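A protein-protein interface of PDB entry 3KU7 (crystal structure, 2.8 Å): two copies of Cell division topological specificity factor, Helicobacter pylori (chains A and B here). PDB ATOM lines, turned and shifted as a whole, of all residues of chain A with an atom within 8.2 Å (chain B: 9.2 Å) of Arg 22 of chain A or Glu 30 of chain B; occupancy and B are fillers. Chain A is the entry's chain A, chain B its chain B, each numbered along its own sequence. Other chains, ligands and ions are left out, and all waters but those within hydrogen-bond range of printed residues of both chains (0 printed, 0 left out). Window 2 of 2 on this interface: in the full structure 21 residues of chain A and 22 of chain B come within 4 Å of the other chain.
NH1 of Arg 22 of chain A lies within salt-bridge range of OE2 of Glu 30 of chain B, 3.8 Å away. N of Ala 28 of chain B is in hydrogen-bond range of O of Lys 24 of chain A, at 2.7 Å.
The guanidinium group (NH2) of Arg 22 of chain A is in hydrogen-bond range of the backbone carbonyl oxygen (O) of Ala 19 of chain A, 3.1 Å away. NE of Arg 22 of chain A lies within hydrogen-bond range of O of Thr 20 of chain A, at 3.3 Å. The backbone NH (N) of Leu 78 of chain A sits at hydrogen-bond distance from the backbone carbonyl oxygen (O) of Asp 21 of chain A. The backbone NH (N) of Leu 23 of chain A sits at hydrogen-bond distance from the backbone carbonyl oxygen (O) of Ile 76 of chain A. The backbone carbonyl oxygen of Leu 33 of chain B sits close to the side-chain amino group of Lys 29 of chain B. The side-chain carboxylate (OE2) of Glu 70 of chain B is in salt-bridge range of the side-chain amino group (NZ) of Lys 29 of chain B, at 3.7 Å.
Among the printed residues, pairs that only touch across the chains: Asp 21 of chain A with Glu 30 of chain B (3.8 Å), Leu 23 of chain A with Leu 27 of chain B (3.6 Å), Leu 23 of chain A with Ala 28 of chain B (3.5 Å), Leu 23 of chain A with Lys 29 of chain B (3.3 Å), Leu 23 of chain A with Leu 35 of chain B (3.9 Å) and Lys 24 of chain A with Leu 27 of chain B (3.2 Å).
Thr 20 of chain A touches none of the printed residues of chain B. Of chain B, only Glu 30 comes within 4 Å of Arg 22 of chain A. Of the printed residues of chain A, Leu 27 of chain B touches Leu 23 (3.6 Å) and Lys 24 (3.2 Å). Of the printed residues of chain A, Ala 28 of chain B touches Leu 23 and Lys 24. Lys 29 of chain B touches just one residue of chain A: Leu 23. Of chain A, only Asp 21 and Arg 22 come within 4 Å of Glu 30 of chain B. Of the printed residues of chain A, Leu 35 of chain B touches Leu 23. Met 38 of chain B touches none of the printed residues of chain A. The nearest residue of chain B that does not touch Arg 22 of chain A is Lys 29 of chain B (4.5 Å). The nearest residue of chain A that does not touch Glu 30 of chain B is Thr 20 of chain A (4.9 Å).
Of the 16 printed residues of chain B, 5 touch a printed residue of chain A. Hydrophobic or aromatic side chains of chain B within 4 Å of the printed part of chain A: Leu 27, Ala 28 and Leu 35. Along chain B the printed residues that touch a printed residue of chain A span positions 27 to 35. Among the printed residues, 8 pairs touch across the chains. Among the printed residues, Asp or Glu carboxylates within 4 Å of a Lys or Arg side-chain nitrogen of the other chain: Arg 22 of chain A with Glu 30 of chain B.
No position is printed for both chains. Of the 8 pairs that touch across the chains among the printed residues, none has its exchanged pair printed and touching as well.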
ATOM      1  N   ALA A  16      -1.459  33.811  -2.205  1.00  0.00           N
ATOM      2  CA  ALA A  16      -0.421  34.825  -1.893  1.00  0.00           C
ATOM      3  C   ALA A  16       0.756  34.736  -2.857  1.00  0.00           C
ATOM      4  O   ALA A  16       0.754  33.937  -3.794  1.00  0.00           O
ATOM      5  CB  ALA A  16       0.055  34.654  -0.454  1.00  0.00           C
ATOM      6  N   ALA A  17       1.763  35.561  -2.613  1.00  0.00           N
ATOM      7  CA  ALA A  17       2.936  35.594  -3.466  1.00  0.00           C
ATOM      8  C   ALA A  17       3.932  34.505  -3.100  1.00  0.00           C
ATOM      9  O   ALA A  17       5.113  34.782  -2.895  1.00  0.00           O
ATOM     10  CB  ALA A  17       3.598  36.965  -3.377  1.00  0.00           C
ATOM     11  N   THR A  18       3.457  33.262  -3.022  1.00  0.00           N
ATOM     12  CA  THR A  18       4.344  32.156  -2.671  1.00  0.00           C
ATOM     13  C   THR A  18       3.842  30.724  -2.959  1.00  0.00           C
ATOM     14  O   THR A  18       4.522  29.953  -3.643  1.00  0.00           O
ATOM     15  CB  THR A  18       4.774  32.244  -1.168  1.00  0.00           C
ATOM     16  OG1 THR A  18       4.133  33.361  -0.533  1.00  0.00           O
ATOM     17  CG2 THR A  18       6.294  32.412  -1.054  1.00  0.00           C
ATOM     18  N   ALA A  19       2.664  30.367  -2.451  1.00  0.00           N
ATOM     19  CA  ALA A  19       2.134  29.020  -2.656  1.00  0.00           C
ATOM     20  C   ALA A  19       1.632  28.789  -4.078  1.00  0.00           C
ATOM     21  O   ALA A  19       0.998  29.655  -4.676  1.00  0.00           O
ATOM     22  CB  ALA A  19       1.019  28.741  -1.658  1.00  0.00           C
ATOM     23  N   THR A  20       1.930  27.602  -4.601  1.00  0.00           N
ATOM     24  CA  THR A  20       1.541  27.190  -5.951  1.00  0.00           C
ATOM     25  C   THR A  20       2.510  27.688  -7.013  1.00  0.00           C
ATOM     26  O   THR A  20       2.606  28.887  -7.283  1.00  0.00           O
ATOM     27  CB  THR A  20       0.108  27.667  -6.313  1.00  0.00           C
ATOM     28  OG1 THR A  20      -0.849  26.800  -5.697  1.00  0.00           O
ATOM     29  CG2 THR A  20      -0.111  27.666  -7.828  1.00  0.00           C
ATOM     30  N   ASP A  21       3.233  26.753  -7.613  1.00  0.00           N
ATOM     31  CA  ASP A  21       4.186  27.088  -8.657  1.00  0.00           C
ATOM     32  C   ASP A  21       3.544  26.938 -10.014  1.00  0.00           C
ATOM     33  O   ASP A  21       3.028  25.878 -10.371  1.00  0.00           O
ATOM     34  CB  ASP A  21       5.408  26.189  -8.566  1.00  0.00           C
ATOM     35  CG  ASP A  21       6.294  26.546  -7.402  1.00  0.00           C
ATOM     36  OD1 ASP A  21       6.868  27.655  -7.411  1.00  0.00           O
ATOM     37  OD2 ASP A  21       6.408  25.722  -6.472  1.00  0.00           O
ATOM     38  N   ARG A  22       3.584  28.016 -10.774  1.00  0.00           N
ATOM     39  CA  ARG A  22       2.983  28.036 -12.085  1.00  0.00           C
ATOM     40  C   ARG A  22       4.062  28.105 -13.162  1.00  0.00           C
ATOM     41  O   ARG A  22       5.209  28.449 -12.892  1.00  0.00           O
ATOM     42  CB  ARG A  22       2.038  29.251 -12.162  1.00  0.00           C
ATOM     43  CG  ARG A  22       1.076  29.379 -10.954  1.00  0.00           C
ATOM     44  CD  ARG A  22       1.021  30.817 -10.383  1.00  0.00           C
ATOM     45  NE  ARG A  22       0.586  30.892  -8.974  1.00  0.00           N
ATOM     46  CZ  ARG A  22       1.030  31.788  -8.087  1.00  0.00           C
ATOM     47  NH1 ARG A  22       1.933  32.697  -8.439  1.00  0.00           N
ATOM     48  NH2 ARG A  22       0.563  31.782  -6.842  1.00  0.00           N
ATOM     49  N   LEU A  23       3.671  27.742 -14.377  1.00  0.00           N
ATOM     50  CA  LEU A  23       4.517  27.774 -15.561  1.00  0.00           C
ATOM     51  C   LEU A  23       3.542  28.305 -16.613  1.00  0.00           C
ATOM     52  O   LEU A  23       2.366  27.969 -16.573  1.00  0.00           O
ATOM     53  CB  LEU A  23       4.984  26.364 -15.907  1.00  0.00           C
ATOM     54  CG  LEU A  23       6.287  26.198 -16.680  1.00  0.00           C
ATOM     55  CD1 LEU A  23       7.481  26.662 -15.854  1.00  0.00           C
ATOM     56  CD2 LEU A  23       6.427  24.733 -17.008  1.00  0.00           C
ATOM     57  N   LYS A  24       4.027  29.122 -17.546  1.00  0.00           N
ATOM     58  CA  LYS A  24       3.176  29.719 -18.573  1.00  0.00           C
ATOM     59  C   LYS A  24       3.732  29.579 -19.978  1.00  0.00           C
ATOM     60  O   LYS A  24       4.876  29.887 -20.230  1.00  0.00           O
ATOM     61  CB  LYS A  24       2.972  31.200 -18.258  1.00  0.00           C
ATOM     62  CG  LYS A  24       2.134  31.946 -19.273  1.00  0.00           C
ATOM     63  CD  LYS A  24       0.813  32.368 -18.652  1.00  0.00           C
ATOM     64  CE  LYS A  24       0.232  33.607 -19.351  1.00  0.00           C
ATOM     65  NZ  LYS A  24      -0.706  34.387 -18.486  1.00  0.00           N
ATOM     66  N   LEU A  25       2.887  29.159 -20.905  1.00  0.00           N
ATOM     67  CA  LEU A  25       3.296  28.971 -22.286  1.00  0.00           C
ATOM     68  C   LEU A  25       2.427  29.744 -23.258  1.00  0.00           C
ATOM     69  O   LEU A  25       1.207  29.650 -23.222  1.00  0.00           O
ATOM     70  CB  LEU A  25       3.249  27.484 -22.622  1.00  0.00           C
ATOM     71  CG  LEU A  25       3.332  27.151 -24.093  1.00  0.00           C
ATOM     72  CD1 LEU A  25       4.775  27.142 -24.539  1.00  0.00           C
ATOM     73  CD2 LEU A  25       2.711  25.796 -24.282  1.00  0.00           C
ATOM     74  N   ASP A  57      -2.820  19.877 -13.743  1.00  0.00           N
ATOM     75  CA  ASP A  57      -3.705  21.037 -13.731  1.00  0.00           C
ATOM     76  C   ASP A  57      -3.267  21.904 -14.899  1.00  0.00           C
ATOM     77  O   ASP A  57      -2.284  22.623 -14.816  1.00  0.00           O
ATOM     78  CB  ASP A  57      -3.578  21.821 -12.412  1.00  0.00           C
ATOM     79  CG  ASP A  57      -4.472  23.081 -12.362  1.00  0.00           C
ATOM     80  OD1 ASP A  57      -4.758  23.553 -11.237  1.00  0.00           O
ATOM     81  OD2 ASP A  57      -4.876  23.619 -13.419  1.00  0.00           O
ATOM     82  N   VAL A  74      -1.428  29.059 -22.271  1.00  0.00           N
ATOM     83  CA  VAL A  74      -1.524  27.839 -21.477  1.00  0.00           C
ATOM     84  C   VAL A  74      -0.881  27.958 -20.101  1.00  0.00           C
ATOM     85  O   VAL A  74       0.342  28.061 -19.991  1.00  0.00           O
ATOM     86  CB  VAL A  74      -0.870  26.640 -22.191  1.00  0.00           C
ATOM     87  CG1 VAL A  74      -0.896  25.435 -21.284  1.00  0.00           C
ATOM     88  CG2 VAL A  74      -1.621  26.312 -23.439  1.00  0.00           C
ATOM     89  N   GLU A  75      -1.721  27.922 -19.062  1.00  0.00           N
ATOM     90  CA  GLU A  75      -1.280  28.013 -17.678  1.00  0.00           C
ATOM     91  C   GLU A  75      -1.165  26.625 -17.083  1.00  0.00           C
ATOM     92  O   GLU A  75      -2.082  25.808 -17.111  1.00  0.00           O
ATOM     93  CB  GLU A  75      -2.243  28.876 -16.856  1.00  0.00           C
ATOM     94  CG  GLU A  75      -2.347  30.321 -17.324  1.00  0.00           C
ATOM     95  CD  GLU A  75      -3.085  30.522 -18.674  1.00  0.00           C
ATOM     96  OE1 GLU A  75      -2.944  31.612 -19.271  1.00  0.00           O
ATOM     97  OE2 GLU A  75      -3.819  29.621 -19.143  1.00  0.00           O
ATOM     98  N   ILE A  76       0.003  26.393 -16.518  1.00  0.00           N
ATOM     99  CA  ILE A  76       0.353  25.119 -15.947  1.00  0.00           C
ATOM    100  C   ILE A  76       0.786  25.185 -14.486  1.00  0.00           C
ATOM    101  O   ILE A  76       1.802  25.776 -14.154  1.00  0.00           O
ATOM    102  CB  ILE A  76       1.495  24.510 -16.795  1.00  0.00           C
ATOM    103  CG1 ILE A  76       1.091  24.512 -18.286  1.00  0.00           C
ATOM    104  CG2 ILE A  76       1.827  23.117 -16.283  1.00  0.00           C
ATOM    105  CD1 ILE A  76       2.232  24.317 -19.283  1.00  0.00           C
ATOM    106  N   ILE A  77       0.006  24.556 -13.620  1.00  0.00           N
ATOM    107  CA  ILE A  77       0.327  24.505 -12.207  1.00  0.00           C
ATOM    108  C   ILE A  77       1.180  23.279 -11.919  1.00  0.00           C
ATOM    109  O   ILE A  77       0.750  22.157 -12.139  1.00  0.00           O
ATOM    110  CB  ILE A  77      -0.947  24.434 -11.348  1.00  0.00           C
ATOM    111  CG1 ILE A  77      -1.669  25.776 -11.350  1.00  0.00           C
ATOM    112  CG2 ILE A  77      -0.600  24.057  -9.960  1.00  0.00           C
ATOM    113  CD1 ILE A  77      -2.354  26.062 -12.652  1.00  0.00           C
ATOM    114  N   LEU A  78       2.387  23.501 -11.407  1.00  0.00           N
ATOM    115  CA  LEU A  78       3.301  22.407 -11.074  1.00  0.00           C
ATOM    116  C   LEU A  78       2.905  21.643  -9.812  1.00  0.00           C
ATOM    117  O   LEU A  78       2.276  22.189  -8.909  1.00  0.00           O
ATOM    118  CB  LEU A  78       4.736  22.926 -10.905  1.00  0.00           C
ATOM    119  CG  LEU A  78       5.417  23.625 -12.077  1.00  0.00           C
ATOM    120  CD1 LEU A  78       6.866  23.970 -11.717  1.00  0.00           C
ATOM    121  CD2 LEU A  78       5.358  22.725 -13.287  1.00  0.00           C
ATOM    122  N   PRO A  79       3.273  20.360  -9.740  1.00  0.00           N
ATOM    123  CA  PRO A  79       2.959  19.515  -8.590  1.00  0.00           C
ATOM    124  C   PRO A  79       3.700  19.908  -7.308  1.00  0.00           C
ATOM    125  O   PRO A  79       4.928  20.015  -7.280  1.00  0.00           O
ATOM    126  CB  PRO A  79       3.334  18.122  -9.083  1.00  0.00           C
ATOM    127  CG  PRO A  79       3.112  18.224 -10.578  1.00  0.00           C
ATOM    128  CD  PRO A  79       3.736  19.545 -10.876  1.00  0.00           C
ATOM    129  N   LEU B  27       7.844  30.367 -22.856  1.00  0.00           N
ATOM    130  CA  LEU B  27       7.696  29.444 -21.742  1.00  0.00           C
ATOM    131  C   LEU B  27       8.249  30.271 -20.609  1.00  0.00           C
ATOM    132  O   LEU B  27       9.439  30.557 -20.547  1.00  0.00           O
ATOM    133  CB  LEU B  27       8.526  28.171 -21.924  1.00  0.00           C
ATOM    134  CG  LEU B  27       7.834  26.887 -21.423  1.00  0.00           C
ATOM    135  CD1 LEU B  27       8.771  25.723 -21.492  1.00  0.00           C
ATOM    136  CD2 LEU B  27       7.398  27.030 -19.993  1.00  0.00           C
ATOM    137  N   ALA B  28       7.354  30.699 -19.734  1.00  0.00           N
ATOM    138  CA  ALA B  28       7.721  31.530 -18.608  1.00  0.00           C
ATOM    139  C   ALA B  28       7.606  30.839 -17.265  1.00  0.00           C
ATOM    140  O   ALA B  28       6.728  30.006 -17.045  1.00  0.00           O
ATOM    141  CB  ALA B  28       6.874  32.776 -18.612  1.00  0.00           C
ATOM    142  N   LYS B  29       8.528  31.191 -16.375  1.00  0.00           N
ATOM    143  CA  LYS B  29       8.548  30.653 -15.029  1.00  0.00           C
ATOM    144  C   LYS B  29       9.224  31.661 -14.119  1.00  0.00           C
ATOM    145  O   LYS B  29       9.836  32.629 -14.569  1.00  0.00           O
ATOM    146  CB  LYS B  29       9.295  29.319 -14.966  1.00  0.00           C
ATOM    147  CG  LYS B  29      10.809  29.422 -14.965  1.00  0.00           C
ATOM    148  CD  LYS B  29      11.420  28.095 -14.582  1.00  0.00           C
ATOM    149  CE  LYS B  29      12.470  28.253 -13.486  1.00  0.00           C
ATOM    150  NZ  LYS B  29      13.782  28.775 -13.950  1.00  0.00           N
ATOM    151  N   GLU B  30       9.084  31.445 -12.826  1.00  0.00           N
ATOM    152  CA  GLU B  30       9.694  32.337 -11.870  1.00  0.00           C
ATOM    153  C   GLU B  30      11.133  31.862 -11.828  1.00  0.00           C
ATOM    154  O   GLU B  30      11.389  30.671 -11.640  1.00  0.00           O
ATOM    155  CB  GLU B  30       8.954  32.207 -10.537  1.00  0.00           C
ATOM    156  CG  GLU B  30       7.488  32.703 -10.641  1.00  0.00           C
ATOM    157  CD  GLU B  30       6.512  31.997  -9.684  1.00  0.00           C
ATOM    158  OE1 GLU B  30       6.535  30.746  -9.632  1.00  0.00           O
ATOM    159  OE2 GLU B  30       5.705  32.685  -9.003  1.00  0.00           O
ATOM    160  N   ARG B  31      12.060  32.789 -12.051  1.00  0.00           N
ATOM    161  CA  ARG B  31      13.483  32.482 -12.093  1.00  0.00           C
ATOM    162  C   ARG B  31      14.064  31.793 -10.869  1.00  0.00           C
ATOM    163  O   ARG B  31      15.085  31.110 -10.978  1.00  0.00           O
ATOM    164  CB  ARG B  31      14.279  33.751 -12.366  1.00  0.00           C
ATOM    165  CG  ARG B  31      15.777  33.531 -12.309  1.00  0.00           C
ATOM    166  CD  ARG B  31      16.555  34.768 -12.727  1.00  0.00           C
ATOM    167  NE  ARG B  31      17.455  35.236 -11.669  1.00  0.00           N
ATOM    168  CZ  ARG B  31      18.585  35.913 -11.876  1.00  0.00           C
ATOM    169  NH1 ARG B  31      18.974  36.209 -13.111  1.00  0.00           N
ATOM    170  NH2 ARG B  31      19.327  36.298 -10.844  1.00  0.00           N
ATOM    171  N   THR B  32      13.446  32.001  -9.707  1.00  0.00           N
ATOM    172  CA  THR B  32      13.900  31.370  -8.462  1.00  0.00           C
ATOM    173  C   THR B  32      13.770  29.851  -8.616  1.00  0.00           C
ATOM    174  O   THR B  32      14.750  29.112  -8.515  1.00  0.00           O
ATOM    175  CB  THR B  32      13.041  31.838  -7.231  1.00  0.00           C
ATOM    176  OG1 THR B  32      13.662  32.973  -6.610  1.00  0.00           O
ATOM    177  CG2 THR B  32      12.875  30.695  -6.190  1.00  0.00           C
ATOM    178  N   LEU B  33      12.539  29.413  -8.860  1.00  0.00           N
ATOM    179  CA  LEU B  33      12.163  28.016  -9.033  1.00  0.00           C
ATOM    180  C   LEU B  33      13.158  27.154  -9.819  1.00  0.00           C
ATOM    181  O   LEU B  33      13.530  27.462 -10.947  1.00  0.00           O
ATOM    182  CB  LEU B  33      10.773  27.990  -9.671  1.00  0.00           C
ATOM    183  CG  LEU B  33      10.006  26.683  -9.769  1.00  0.00           C
ATOM    184  CD1 LEU B  33      10.190  26.156 -11.150  1.00  0.00           C
ATOM    185  CD2 LEU B  33      10.464  25.692  -8.711  1.00  0.00           C
ATOM    186  N   ASN B  34      13.561  26.047  -9.207  1.00  0.00           N
ATOM    187  CA  ASN B  34      14.532  25.130  -9.788  1.00  0.00           C
ATOM    188  C   ASN B  34      13.918  24.003 -10.602  1.00  0.00           C
ATOM    189  O   ASN B  34      13.341  23.074 -10.046  1.00  0.00           O
ATOM    190  CB  ASN B  34      15.389  24.539  -8.673  1.00  0.00           C
ATOM    191  CG  ASN B  34      16.462  23.619  -9.194  1.00  0.00           C
ATOM    192  OD1 ASN B  34      16.172  22.557  -9.739  1.00  0.00           O
ATOM    193  ND2 ASN B  34      17.715  24.026  -9.035  1.00  0.00           N
ATOM    194  N   LEU B  35      14.057  24.088 -11.923  1.00  0.00           N
ATOM    195  CA  LEU B  35      13.522  23.070 -12.819  1.00  0.00           C
ATOM    196  C   LEU B  35      14.606  22.393 -13.621  1.00  0.00           C
ATOM    197  O   LEU B  35      14.971  22.832 -14.712  1.00  0.00           O
ATOM    198  CB  LEU B  35      12.491  23.664 -13.763  1.00  0.00           C
ATOM    199  CG  LEU B  35      11.259  24.121 -12.996  1.00  0.00           C
ATOM    200  CD1 LEU B  35      10.162  24.458 -13.979  1.00  0.00           C
ATOM    201  CD2 LEU B  35      10.806  23.030 -12.024  1.00  0.00           C
ATOM    202  N   TYR B  37      14.699  19.901 -15.502  1.00  0.00           N
ATOM    203  CA  TYR B  37      14.311  19.484 -16.845  1.00  0.00           C
ATOM    204  C   TYR B  37      14.093  20.571 -17.872  1.00  0.00           C
ATOM    205  O   TYR B  37      13.868  20.261 -19.045  1.00  0.00           O
ATOM    206  CB  TYR B  37      13.067  18.617 -16.755  1.00  0.00           C
ATOM    207  CG  TYR B  37      12.008  19.236 -15.890  1.00  0.00           C
ATOM    208  CD1 TYR B  37      11.268  20.329 -16.335  1.00  0.00           C
ATOM    209  CD2 TYR B  37      11.745  18.734 -14.617  1.00  0.00           C
ATOM    210  CE1 TYR B  37      10.292  20.920 -15.528  1.00  0.00           C
ATOM    211  CE2 TYR B  37      10.770  19.315 -13.796  1.00  0.00           C
ATOM    212  CZ  TYR B  37      10.041  20.399 -14.262  1.00  0.00           C
ATOM    213  OH  TYR B  37       9.057  20.933 -13.460  1.00  0.00           O
ATOM    214  N   MET B  38      14.109  21.833 -17.437  1.00  0.00           N
ATOM    215  CA  MET B  38      13.982  22.937 -18.381  1.00  0.00           C
ATOM    216  C   MET B  38      15.162  22.579 -19.243  1.00  0.00           C
ATOM    217  O   MET B  38      16.114  21.990 -18.739  1.00  0.00           O
ATOM    218  CB  MET B  38      14.255  24.293 -17.716  1.00  0.00           C
ATOM    219  CG  MET B  38      13.119  24.901 -16.922  1.00  0.00           C
ATOM    220  SD  MET B  38      11.693  25.409 -17.938  1.00  0.00           S
ATOM    221  CE  MET B  38      12.439  26.434 -19.208  1.00  0.00           C
ATOM    222  N   LEU B  63      15.750  34.947 -21.428  1.00  0.00           N
ATOM    223  CA  LEU B  63      15.862  36.322 -20.959  1.00  0.00           C
ATOM    224  C   LEU B  63      15.731  36.442 -19.438  1.00  0.00           C
ATOM    225  O   LEU B  63      14.772  35.954 -18.840  1.00  0.00           O
ATOM    226  CB  LEU B  63      14.817  37.211 -21.656  1.00  0.00           C
ATOM    227  CG  LEU B  63      14.841  37.254 -23.193  1.00  0.00           C
ATOM    228  CD1 LEU B  63      13.945  38.390 -23.681  1.00  0.00           C
ATOM    229  CD2 LEU B  63      16.266  37.471 -23.690  1.00  0.00           C
ATOM    230  N   SER B  68      13.602  37.584 -11.743  1.00  0.00           N
ATOM    231  CA  SER B  68      12.233  37.577 -11.241  1.00  0.00           C
ATOM    232  C   SER B  68      11.386  36.639 -12.101  1.00  0.00           C
ATOM    233  O   SER B  68      10.573  35.870 -11.575  1.00  0.00           O
ATOM    234  CB  SER B  68      11.666  39.004 -11.262  1.00  0.00           C
ATOM    235  OG  SER B  68      10.432  39.096 -10.566  1.00  0.00           O
ATOM    236  N   VAL B  69      11.578  36.704 -13.417  1.00  0.00           N
ATOM    237  CA  VAL B  69      10.851  35.840 -14.346  1.00  0.00           C
ATOM    238  C   VAL B  69      11.712  35.384 -15.520  1.00  0.00           C
ATOM    239  O   VAL B  69      12.065  36.201 -16.365  1.00  0.00           O
ATOM    240  CB  VAL B  69       9.644  36.551 -14.937  1.00  0.00           C
ATOM    241  CG1 VAL B  69       9.188  35.846 -16.207  1.00  0.00           C
ATOM    242  CG2 VAL B  69       8.529  36.561 -13.945  1.00  0.00           C
ATOM    243  N   GLU B  70      12.045  34.091 -15.579  1.00  0.00           N
ATOM    244  CA  GLU B  70      12.845  33.562 -16.688  1.00  0.00           C
ATOM    245  C   GLU B  70      11.917  33.106 -17.800  1.00  0.00           C
ATOM    246  O   GLU B  70      11.001  32.306 -17.601  1.00  0.00           O
ATOM    247  CB  GLU B  70      13.716  32.382 -16.282  1.00  0.00           C
ATOM    248  CG  GLU B  70      14.269  31.650 -17.512  1.00  0.00           C
ATOM    249  CD  GLU B  70      14.965  30.351 -17.174  1.00  0.00           C
ATOM    250  OE1 GLU B  70      14.503  29.288 -17.667  1.00  0.00           O
ATOM    251  OE2 GLU B  70      15.968  30.396 -16.422  1.00  0.00           O
ATOM    252  N   THR B  71      12.186  33.607 -18.988  1.00  0.00           N
ATOM    253  CA  THR B  71      11.358  33.306 -20.123  1.00  0.00           C
ATOM    254  C   THR B  71      12.195  32.704 -21.226  1.00  0.00           C
ATOM    255  O   THR B  71      13.281  33.192 -21.504  1.00  0.00           O
ATOM    256  CB  THR B  71      10.694  34.609 -20.601  1.00  0.00           C
ATOM    257  OG1 THR B  71       9.293  34.406 -20.711  1.00  0.00           O
ATOM    258  CG2 THR B  71      11.227  35.053 -21.948  1.00  0.00           C
